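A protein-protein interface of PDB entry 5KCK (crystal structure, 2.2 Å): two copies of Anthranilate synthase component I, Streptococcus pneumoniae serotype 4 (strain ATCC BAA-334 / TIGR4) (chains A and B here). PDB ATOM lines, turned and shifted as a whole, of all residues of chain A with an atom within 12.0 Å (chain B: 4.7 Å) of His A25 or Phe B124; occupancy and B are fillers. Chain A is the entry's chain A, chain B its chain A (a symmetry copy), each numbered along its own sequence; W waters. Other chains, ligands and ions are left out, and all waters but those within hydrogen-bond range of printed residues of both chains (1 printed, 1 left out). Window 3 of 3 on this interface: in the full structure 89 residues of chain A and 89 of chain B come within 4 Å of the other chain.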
ATOM      1  N   ALA A  17      -6.128   4.088 -14.464  1.00  0.00           N
ATOM      2  CA  ALA A  17      -5.017   4.943 -14.062  1.00  0.00           C
ATOM      3  C   ALA A  17      -3.848   4.796 -15.026  1.00  0.00           C
ATOM      4  O   ALA A  17      -3.276   5.794 -15.485  1.00  0.00           O
ATOM      5  CB  ALA A  17      -4.589   4.620 -12.627  1.00  0.00           C
ATOM      6  N   TYR A  18      -3.493   3.554 -15.366  1.00  0.00           N
ATOM      7  CA  TYR A  18      -2.359   3.330 -16.261  1.00  0.00           C
ATOM      8  C   TYR A  18      -2.569   4.018 -17.605  1.00  0.00           C
ATOM      9  O   TYR A  18      -1.663   4.681 -18.126  1.00  0.00           O
ATOM     10  CB  TYR A  18      -2.138   1.835 -16.460  1.00  0.00           C
ATOM     11  CG  TYR A  18      -0.789   1.504 -17.052  1.00  0.00           C
ATOM     12  CD1 TYR A  18      -0.573   1.521 -18.429  1.00  0.00           C
ATOM     13  CD2 TYR A  18       0.273   1.190 -16.230  1.00  0.00           C
ATOM     14  CE1 TYR A  18       0.675   1.213 -18.958  1.00  0.00           C
ATOM     15  CE2 TYR A  18       1.508   0.868 -16.743  1.00  0.00           C
ATOM     16  CZ  TYR A  18       1.710   0.890 -18.103  1.00  0.00           C
ATOM     17  OH  TYR A  18       2.959   0.580 -18.577  1.00  0.00           O
ATOM     18  N   MET A  19      -3.761   3.877 -18.178  1.00  0.00           N
ATOM     19  CA  MET A  19      -4.046   4.449 -19.487  1.00  0.00           C
ATOM     20  C   MET A  19      -4.015   5.976 -19.482  1.00  0.00           C
ATOM     21  O   MET A  19      -3.675   6.594 -20.488  1.00  0.00           O
ATOM     22  CB  MET A  19      -5.408   3.971 -19.989  1.00  0.00           C
ATOM     23  CG  MET A  19      -5.479   2.490 -20.313  1.00  0.00           C
ATOM     24  SD  MET A  19      -7.326   1.906 -20.730  1.00  0.00           S
ATOM     25  CE  MET A  19      -6.874   0.536 -22.043  1.00  0.00           C
ATOM     26  N   ARG A  20      -4.387   6.583 -18.351  1.00  0.00           N
ATOM     27  CA  ARG A  20      -4.492   8.037 -18.266  1.00  0.00           C
ATOM     28  C   ARG A  20      -3.202   8.706 -17.809  1.00  0.00           C
ATOM     29  O   ARG A  20      -2.963   9.867 -18.163  1.00  0.00           O
ATOM     30  CB  ARG A  20      -5.630   8.433 -17.315  1.00  0.00           C
ATOM     31  CG  ARG A  20      -7.025   8.007 -17.786  1.00  0.00           C
ATOM     32  CD  ARG A  20      -8.096   8.347 -16.758  1.00  0.00           C
ATOM     33  NE  ARG A  20      -9.401   7.808 -17.131  1.00  0.00           N
ATOM     34  CZ  ARG A  20     -10.497   7.892 -16.376  1.00  0.00           C
ATOM     35  NH1 ARG A  20     -10.445   8.493 -15.196  1.00  0.00           N
ATOM     36  NH2 ARG A  20     -11.647   7.368 -16.801  1.00  0.00           N
ATOM     37  N   LEU A  21      -2.376   8.017 -17.025  1.00  0.00           N
ATOM     38  CA  LEU A  21      -1.158   8.632 -16.519  1.00  0.00           C
ATOM     39  C   LEU A  21      -0.180   8.890 -17.653  1.00  0.00           C
ATOM     40  O   LEU A  21      -0.034   8.080 -18.572  1.00  0.00           O
ATOM     41  CB  LEU A  21      -0.515   7.751 -15.452  1.00  0.00           C
ATOM     42  CG  LEU A  21      -1.258   7.822 -14.113  1.00  0.00           C
ATOM     43  CD1 LEU A  21      -0.603   6.952 -13.073  1.00  0.00           C
ATOM     44  CD2 LEU A  21      -1.370   9.259 -13.627  1.00  0.00           C
ATOM     45  N   LYS A  22       0.496  10.031 -17.582  1.00  0.00           N
ATOM     46  CA  LYS A  22       1.426  10.446 -18.623  1.00  0.00           C
ATOM     47  C   LYS A  22       2.883  10.358 -18.192  1.00  0.00           C
ATOM     48  O   LYS A  22       3.761  10.770 -18.953  1.00  0.00           O
ATOM     49  CB  LYS A  22       1.096  11.868 -19.069  1.00  0.00           C
ATOM     50  CG  LYS A  22      -0.336  12.010 -19.568  1.00  0.00           C
ATOM     51  CD  LYS A  22      -0.544  11.202 -20.843  1.00  0.00           C
ATOM     52  CE  LYS A  22      -1.929  11.425 -21.414  1.00  0.00           C
ATOM     53  NZ  LYS A  22      -2.106  10.752 -22.730  1.00  0.00           N
ATOM     54  N   GLY A  23       3.162   9.829 -17.000  1.00  0.00           N
ATOM     55  CA  GLY A  23       4.522   9.760 -16.503  1.00  0.00           C
ATOM     56  C   GLY A  23       5.384   8.731 -17.221  1.00  0.00           C
ATOM     57  O   GLY A  23       4.915   7.858 -17.952  1.00  0.00           O
ATOM     58  N   GLN A  24       6.689   8.850 -16.991  1.00  0.00           N
ATOM     59  CA  GLN A  24       7.678   7.968 -17.593  1.00  0.00           C
ATOM     60  C   GLN A  24       7.764   6.639 -16.843  1.00  0.00           C
ATOM     61  O   GLN A  24       7.492   6.566 -15.642  1.00  0.00           O
ATOM     62  CB  GLN A  24       9.053   8.649 -17.585  1.00  0.00           C
ATOM     63  CG  GLN A  24       9.095   9.984 -18.348  1.00  0.00           C
ATOM     64  CD  GLN A  24      10.406  10.732 -18.152  1.00  0.00           C
ATOM     65  OE1 GLN A  24      11.469  10.125 -18.027  1.00  0.00           O
ATOM     66  NE2 GLN A  24      10.333  12.058 -18.116  1.00  0.00           N
ATOM     67  N   HIS A  25       8.156   5.588 -17.573  1.00  0.00           N
ATOM     68  CA  HIS A  25       8.515   4.271 -17.018  1.00  0.00           C
ATOM     69  C   HIS A  25       7.449   3.724 -16.061  1.00  0.00           C
ATOM     70  O   HIS A  25       7.722   3.402 -14.904  1.00  0.00           O
ATOM     71  CB  HIS A  25       9.877   4.333 -16.318  1.00  0.00           C
ATOM     72  CG  HIS A  25      10.972   4.870 -17.177  1.00  0.00           C
ATOM     73  ND1 HIS A  25      11.455   4.192 -18.275  1.00  0.00           N
ATOM     74  CD2 HIS A  25      11.677   6.026 -17.107  1.00  0.00           C
ATOM     75  CE1 HIS A  25      12.412   4.905 -18.844  1.00  0.00           C
ATOM     76  NE2 HIS A  25      12.562   6.024 -18.157  1.00  0.00           N
ATOM     77  N   LYS A  26       6.219   3.625 -16.570  1.00  0.00           N
ATOM     78  CA  LYS A  26       5.079   3.162 -15.783  1.00  0.00           C
ATOM     79  C   LYS A  26       5.119   1.646 -15.580  1.00  0.00           C
ATOM     80  O   LYS A  26       5.300   0.886 -16.536  1.00  0.00           O
ATOM     81  CB  LYS A  26       3.776   3.555 -16.479  1.00  0.00           C
ATOM     82  CG  LYS A  26       3.425   5.022 -16.353  1.00  0.00           C
ATOM     83  CD  LYS A  26       2.731   5.560 -17.601  1.00  0.00           C
ATOM     84  CE  LYS A  26       1.586   4.678 -18.051  1.00  0.00           C
ATOM     85  NZ  LYS A  26       0.712   5.379 -19.039  1.00  0.00           N
ATOM     86  N   VAL A  27       4.940   1.207 -14.339  1.00  0.00           N
ATOM     87  CA  VAL A  27       4.888  -0.214 -14.006  1.00  0.00           C
ATOM     88  C   VAL A  27       3.628  -0.474 -13.194  1.00  0.00           C
ATOM     89  O   VAL A  27       3.143   0.403 -12.470  1.00  0.00           O
ATOM     90  CB  VAL A  27       6.146  -0.692 -13.226  1.00  0.00           C
ATOM     91  CG1 VAL A  27       7.400  -0.556 -14.080  1.00  0.00           C
ATOM     92  CG2 VAL A  27       6.315   0.066 -11.887  1.00  0.00           C
ATOM     93  N   ILE A  28       3.087  -1.686 -13.331  1.00  0.00           N
ATOM     94  CA  ILE A  28       1.972  -2.163 -12.520  1.00  0.00           C
ATOM     95  C   ILE A  28       2.400  -3.455 -11.856  1.00  0.00           C
ATOM     96  O   ILE A  28       2.887  -4.363 -12.533  1.00  0.00           O
ATOM     97  CB  ILE A  28       0.694  -2.451 -13.332  1.00  0.00           C
ATOM     98  CG1 ILE A  28       0.377  -1.376 -14.333  1.00  0.00           C
ATOM     99  CG2 ILE A  28      -0.504  -2.620 -12.387  1.00  0.00           C
ATOM    100  CD1 ILE A  28      -0.914  -1.678 -15.095  1.00  0.00           C
ATOM    101  N   LEU A  29       2.145  -3.561 -10.558  1.00  0.00           N
ATOM    102  CA  LEU A  29       2.325  -4.789  -9.793  1.00  0.00           C
ATOM    103  C   LEU A  29       1.072  -4.987  -8.953  1.00  0.00           C
ATOM    104  O   LEU A  29       0.645  -4.066  -8.248  1.00  0.00           O
ATOM    105  CB  LEU A  29       3.570  -4.698  -8.909  1.00  0.00           C
ATOM    106  CG  LEU A  29       3.904  -5.846  -7.965  1.00  0.00           C
ATOM    107  CD1 LEU A  29       4.084  -7.171  -8.711  1.00  0.00           C
ATOM    108  CD2 LEU A  29       5.159  -5.483  -7.196  1.00  0.00           C
ATOM    109  N   ALA B  45       3.415   2.699 -10.487  1.00  0.00           N
ATOM    110  CA  ALA B  45       4.527   3.608 -10.222  1.00  0.00           C
ATOM    111  C   ALA B  45       5.012   4.250 -11.513  1.00  0.00           C
ATOM    112  O   ALA B  45       4.963   3.637 -12.584  1.00  0.00           O
ATOM    113  CB  ALA B  45       5.698   2.891  -9.538  1.00  0.00           C
ATOM    114  N   TYR B  46       5.515   5.482 -11.392  1.00  0.00           N
ATOM    115  CA  TYR B  46       5.851   6.298 -12.555  1.00  0.00           C
ATOM    116  C   TYR B  46       6.909   7.327 -12.169  1.00  0.00           C
ATOM    117  O   TYR B  46       7.132   7.607 -10.988  1.00  0.00           O
ATOM    118  CB  TYR B  46       4.600   6.989 -13.122  1.00  0.00           C
ATOM    119  CG  TYR B  46       3.633   7.371 -12.027  1.00  0.00           C
ATOM    120  CD1 TYR B  46       3.751   8.588 -11.356  1.00  0.00           C
ATOM    121  CD2 TYR B  46       2.635   6.494 -11.627  1.00  0.00           C
ATOM    122  CE1 TYR B  46       2.877   8.929 -10.322  1.00  0.00           C
ATOM    123  CE2 TYR B  46       1.767   6.812 -10.590  1.00  0.00           C
ATOM    124  CZ  TYR B  46       1.886   8.028  -9.948  1.00  0.00           C
ATOM    125  OH  TYR B  46       1.010   8.329  -8.929  1.00  0.00           O
ATOM    126  N   PRO B  48      10.370   7.406 -12.273  1.00  0.00           N
ATOM    127  CA  PRO B  48      11.363   6.947 -11.297  1.00  0.00           C
ATOM    128  C   PRO B  48      12.515   7.933 -11.166  1.00  0.00           C
ATOM    129  O   PRO B  48      12.889   8.610 -12.122  1.00  0.00           O
ATOM    130  CB  PRO B  48      11.839   5.617 -11.883  1.00  0.00           C
ATOM    131  CG  PRO B  48      11.704   5.819 -13.363  1.00  0.00           C
ATOM    132  CD  PRO B  48      10.470   6.674 -13.549  1.00  0.00           C
ATOM    133  N   PHE B  50      15.617   6.893 -10.169  1.00  0.00           N
ATOM    134  CA  PHE B  50      16.798   6.147 -10.589  1.00  0.00           C
ATOM    135  C   PHE B  50      16.405   4.931 -11.407  1.00  0.00           C
ATOM    136  O   PHE B  50      15.358   4.309 -11.181  1.00  0.00           O
ATOM    137  CB  PHE B  50      17.633   5.581  -9.423  1.00  0.00           C
ATOM    138  CG  PHE B  50      18.170   6.602  -8.498  1.00  0.00           C
ATOM    139  CD1 PHE B  50      18.967   7.634  -8.966  1.00  0.00           C
ATOM    140  CD2 PHE B  50      17.916   6.506  -7.139  1.00  0.00           C
ATOM    141  CE1 PHE B  50      19.478   8.574  -8.097  1.00  0.00           C
ATOM    142  CE2 PHE B  50      18.421   7.438  -6.262  1.00  0.00           C
ATOM    143  CZ  PHE B  50      19.210   8.476  -6.740  1.00  0.00           C
ATOM    144  N   GLU B  51      17.305   4.571 -12.313  1.00  0.00           N
ATOM    145  CA  GLU B  51      17.341   3.266 -12.954  1.00  0.00           C
ATOM    146  C   GLU B  51      18.603   2.554 -12.491  1.00  0.00           C
ATOM    147  O   GLU B  51      19.705   3.106 -12.595  1.00  0.00           O
ATOM    148  CB  GLU B  51      17.351   3.406 -14.479  1.00  0.00           C
ATOM    149  CG  GLU B  51      17.497   2.100 -15.219  1.00  0.00           C
ATOM    150  CD  GLU B  51      17.723   2.296 -16.710  1.00  0.00           C
ATOM    151  OE1 GLU B  51      18.796   2.811 -17.095  1.00  0.00           O
ATOM    152  OE2 GLU B  51      16.823   1.934 -17.495  1.00  0.00           O
ATOM    153  N   GLY B  92      10.344   2.685  -3.229  1.00  0.00           N
ATOM    154  CA  GLY B  92      11.432   1.749  -3.428  1.00  0.00           C
ATOM    155  C   GLY B  92      11.602   1.295  -4.870  1.00  0.00           C
ATOM    156  O   GLY B  92      11.259   2.033  -5.797  1.00  0.00           O
ATOM    157  N   ALA B  93      12.140   0.090  -5.071  1.00  0.00           N
ATOM    158  CA  ALA B  93      12.501  -0.415  -6.390  1.00  0.00           C
ATOM    159  C   ALA B  93      11.491  -1.442  -6.879  1.00  0.00           C
ATOM    160  O   ALA B  93      11.004  -2.270  -6.105  1.00  0.00           O
ATOM    161  CB  ALA B  93      13.891  -1.056  -6.371  1.00  0.00           C
ATOM    162  N   ILE B  94      11.188  -1.389  -8.170  1.00  0.00           N
ATOM    163  CA  ILE B  94      10.326  -2.361  -8.831  1.00  0.00           C
ATOM    164  C   ILE B  94      11.062  -2.840 -10.073  1.00  0.00           C
ATOM    165  O   ILE B  94      11.604  -2.022 -10.828  1.00  0.00           O
ATOM    166  CB  ILE B  94       8.953  -1.751  -9.182  1.00  0.00           C
ATOM    167  CG1 ILE B  94       8.253  -1.280  -7.898  1.00  0.00           C
ATOM    168  CG2 ILE B  94       8.072  -2.741  -9.969  1.00  0.00           C
ATOM    169  CD1 ILE B  94       6.964  -0.547  -8.142  1.00  0.00           C
ATOM    170  N   HIS B 122      17.334  -5.335 -13.535  1.00  0.00           N
ATOM    171  CA  HIS B 122      16.812  -4.040 -13.952  1.00  0.00           C
ATOM    172  C   HIS B 122      15.746  -3.604 -12.957  1.00  0.00           C
ATOM    173  O   HIS B 122      14.707  -4.262 -12.822  1.00  0.00           O
ATOM    174  CB  HIS B 122      16.240  -4.116 -15.366  1.00  0.00           C
ATOM    175  CG  HIS B 122      16.258  -2.812 -16.100  1.00  0.00           C
ATOM    176  ND1 HIS B 122      16.124  -2.728 -17.470  1.00  0.00           N
ATOM    177  CD2 HIS B 122      16.392  -1.538 -15.656  1.00  0.00           C
ATOM    178  CE1 HIS B 122      16.182  -1.460 -17.838  1.00  0.00           C
ATOM    179  NE2 HIS B 122      16.341  -0.717 -16.756  1.00  0.00           N
ATOM    180  N   PHE B 123      16.002  -2.501 -12.259  1.00  0.00           N
ATOM    181  CA  PHE B 123      15.034  -1.917 -11.345  1.00  0.00           C
ATOM    182  C   PHE B 123      14.858  -0.441 -11.656  1.00  0.00           C
ATOM    183  O   PHE B 123      15.821   0.251 -12.005  1.00  0.00           O
ATOM    184  CB  PHE B 123      15.469  -2.072  -9.872  1.00  0.00           C
ATOM    185  CG  PHE B 123      15.278  -3.455  -9.325  1.00  0.00           C
ATOM    186  CD1 PHE B 123      14.046  -3.849  -8.821  1.00  0.00           C
ATOM    187  CD2 PHE B 123      16.331  -4.363  -9.310  1.00  0.00           C
ATOM    188  CE1 PHE B 123      13.864  -5.127  -8.312  1.00  0.00           C
ATOM    189  CE2 PHE B 123      16.160  -5.644  -8.803  1.00  0.00           C
ATOM    190  CZ  PHE B 123      14.925  -6.030  -8.306  1.00  0.00           C
ATOM    191  N   PHE B 124      13.632   0.035 -11.516  1.00  0.00           N
ATOM    192  CA  PHE B 124      13.374   1.462 -11.413  1.00  0.00           C
ATOM    193  C   PHE B 124      13.079   1.807  -9.953  1.00  0.00           C
ATOM    194  O   PHE B 124      12.464   1.022  -9.223  1.00  0.00           O
ATOM    195  CB  PHE B 124      12.197   1.884 -12.301  1.00  0.00           C
ATOM    196  CG  PHE B 124      12.473   1.837 -13.781  1.00  0.00           C
ATOM    197  CD1 PHE B 124      13.407   2.682 -14.361  1.00  0.00           C
ATOM    198  CD2 PHE B 124      11.744   0.994 -14.604  1.00  0.00           C
ATOM    199  CE1 PHE B 124      13.643   2.659 -15.735  1.00  0.00           C
ATOM    200  CE2 PHE B 124      11.965   0.972 -15.975  1.00  0.00           C
ATOM    201  CZ  PHE B 124      12.921   1.800 -16.540  1.00  0.00           C
ATOM    202  N   VAL B 125      13.503   2.996  -9.534  1.00  0.00           N
ATOM    203  CA  VAL B 125      13.397   3.428  -8.140  1.00  0.00           C
ATOM    204  C   VAL B 125      12.424   4.598  -8.065  1.00  0.00           C
ATOM    205  O   VAL B 125      12.662   5.644  -8.677  1.00  0.00           O
ATOM    206  CB  VAL B 125      14.771   3.808  -7.569  1.00  0.00           C
ATOM    207  CG1 VAL B 125      14.653   4.148  -6.102  1.00  0.00           C
ATOM    208  CG2 VAL B 125      15.765   2.674  -7.801  1.00  0.00           C
ATOM    209  N   TYR B 126      11.344   4.432  -7.300  1.00  0.00           N
ATOM    210  CA  TYR B 126      10.194   5.330  -7.346  1.00  0.00           C
ATOM    211  C   TYR B 126       9.901   5.983  -6.000  1.00  0.00           C
ATOM    212  O   TYR B 126       9.912   5.321  -4.952  1.00  0.00           O
ATOM    213  CB  TYR B 126       8.914   4.596  -7.771  1.00  0.00           C
ATOM    214  CG  TYR B 126       8.945   3.964  -9.137  1.00  0.00           C
ATOM    215  CD1 TYR B 126       8.546   4.673 -10.267  1.00  0.00           C
ATOM    216  CD2 TYR B 126       9.344   2.647  -9.293  1.00  0.00           C
ATOM    217  CE1 TYR B 126       8.556   4.077 -11.524  1.00  0.00           C
ATOM    218  CE2 TYR B 126       9.364   2.049 -10.532  1.00  0.00           C
ATOM    219  CZ  TYR B 126       8.971   2.763 -11.647  1.00  0.00           C
ATOM    220  OH  TYR B 126       8.993   2.148 -12.882  1.00  0.00           O
ATOM    221  N   ASP B 246       7.066  -1.834 -18.030  1.00  0.00           N
ATOM    222  CA  ASP B 246       7.494  -1.211 -19.280  1.00  0.00           C
ATOM    223  C   ASP B 246       8.894  -0.640 -19.080  1.00  0.00           C
ATOM    224  O   ASP B 246       9.061   0.415 -18.467  1.00  0.00           O
ATOM    225  CB  ASP B 246       6.524  -0.126 -19.732  1.00  0.00           C
ATOM    226  CG  ASP B 246       6.855   0.394 -21.130  1.00  0.00           C
ATOM    227  OD1 ASP B 246       7.880  -0.035 -21.705  1.00  0.00           O
ATOM    228  OD2 ASP B 246       6.098   1.235 -21.659  1.00  0.00           O
ATOM    229  N   PHE B 247       9.895  -1.320 -19.632  1.00  0.00           N
ATOM    230  CA  PHE B 247      11.262  -0.832 -19.565  1.00  0.00           C
ATOM    231  C   PHE B 247      11.637  -0.002 -20.784  1.00  0.00           C
ATOM    232  O   PHE B 247      12.805   0.364 -20.935  1.00  0.00           O
ATOM    233  CB  PHE B 247      12.237  -2.003 -19.385  1.00  0.00           C
ATOM    234  CG  PHE B 247      12.147  -2.671 -18.032  1.00  0.00           C
ATOM    235  CD1 PHE B 247      12.782  -2.123 -16.930  1.00  0.00           C
ATOM    236  CD2 PHE B 247      11.430  -3.844 -17.864  1.00  0.00           C
ATOM    237  CE1 PHE B 247      12.704  -2.728 -15.687  1.00  0.00           C
ATOM    238  CE2 PHE B 247      11.352  -4.460 -16.620  1.00  0.00           C
ATOM    239  CZ  PHE B 247      11.988  -3.893 -15.531  1.00  0.00           C
HETATM  240  O   HOH W   1       3.855   1.846 -20.476  1.00  0.00           O
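The backbone carbonyl oxygen of His A25 sits at hydrogen-bond distance from the side-chain hydroxyl of Tyr B126 (2.7 Å). N of Val A27 sits at hydrogen-bond distance from O of Ala B45 (3.0 Å).
The backbone carbonyl oxygen of Gly B92 is in hydrogen-bond range of the backbone NH of Tyr B126, at 2.8 Å. The backbone NH (N) of Ile B94 is in hydrogen-bond range of the backbone carbonyl oxygen (O) of Phe B124 (2.9 Å). NZ of Lys A26 sits at hydrogen-bond distance from O of Tyr A18 (2.6 Å). O of Leu A21 is in hydrogen-bond range of NZ of Lys A26 (2.8 Å).
Tyr A18 touches Asp B246 (OH to CB, 3.8 Å). Leu A21 touches Tyr B46. CA of Tyr B46 touches O of Gln A24, at 3.5 Å. Gln A24 touches Pro B48 (O to CD, 3.6 Å). His A25 touches Ala B45. Pro B48 touches His A25. CA of Lys A26 touches O of Ala B45, at 3.2 Å. Tyr B46 touches Lys A26 (CB to CG, 3.96 Å). Asp B246 touches Lys A26. Val A27 touches Tyr B126.
Of chain B, only Ala B45 (3.6 Å), Pro B48 (3.7 Å), Phe B124 (3.3 Å) and Tyr B126 (2.7 Å) come within 4 Å of His A25. Of chain A, only His A25 comes within 4 Å of Phe B124. Printed residues of chain A within 4 Å of Ala B45: His A25 (3.6 Å), Lys A26 (3.2 Å) and Val A27 (3.0 Å). Pro B48 touches two residues of chain A. Glu B51 touches none of the printed residues of chain A. No residue of chain A comes within 4 Å of Gly B92. No residue of chain A comes within 4 Å of Ala B93. No residue of chain A comes within 4 Å of His B122. No residue of chain A comes within 4 Å of Val B125. Tyr B126 touches just these residues of chain A: His A25 and Val A27. Of the printed residues of chain B, Tyr A18 touches Asp B246 (3.8 Å). Printed residues of chain B within 4 Å of Val A27: Ala B45 (3.0 Å), Ile B94 (3.8 Å) and Tyr B126 (3.4 Å). Of the printed residues of chain B, Leu A21 touches Tyr B46. The nearest printed residue of chain B that does not touch Lys A26 is Tyr B126 (4.7 Å).
Of the 15 printed residues of chain B, 7 touch a printed residue of chain A. Hydrophobic or aromatic side chains of chain B within 4 Å of the printed part of chain A: Ala B45, Tyr B46, Pro B48, Ile B94, Phe B124 and Tyr B126. Of the 13 printed residues of chain A, 6 touch a printed residue of chain B. Among the printed residues, 14 pairs touch across the chains. Among the printed residues, no Asp or Glu carboxylate lies within 4 Å of a Lys or Arg side-chain nitrogen of the other chain.
No position is printed for both chains.
Water W1 bridges OH of Tyr A18 (2.5 Å) and OD2 of Asp B246 (2.6 Å).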
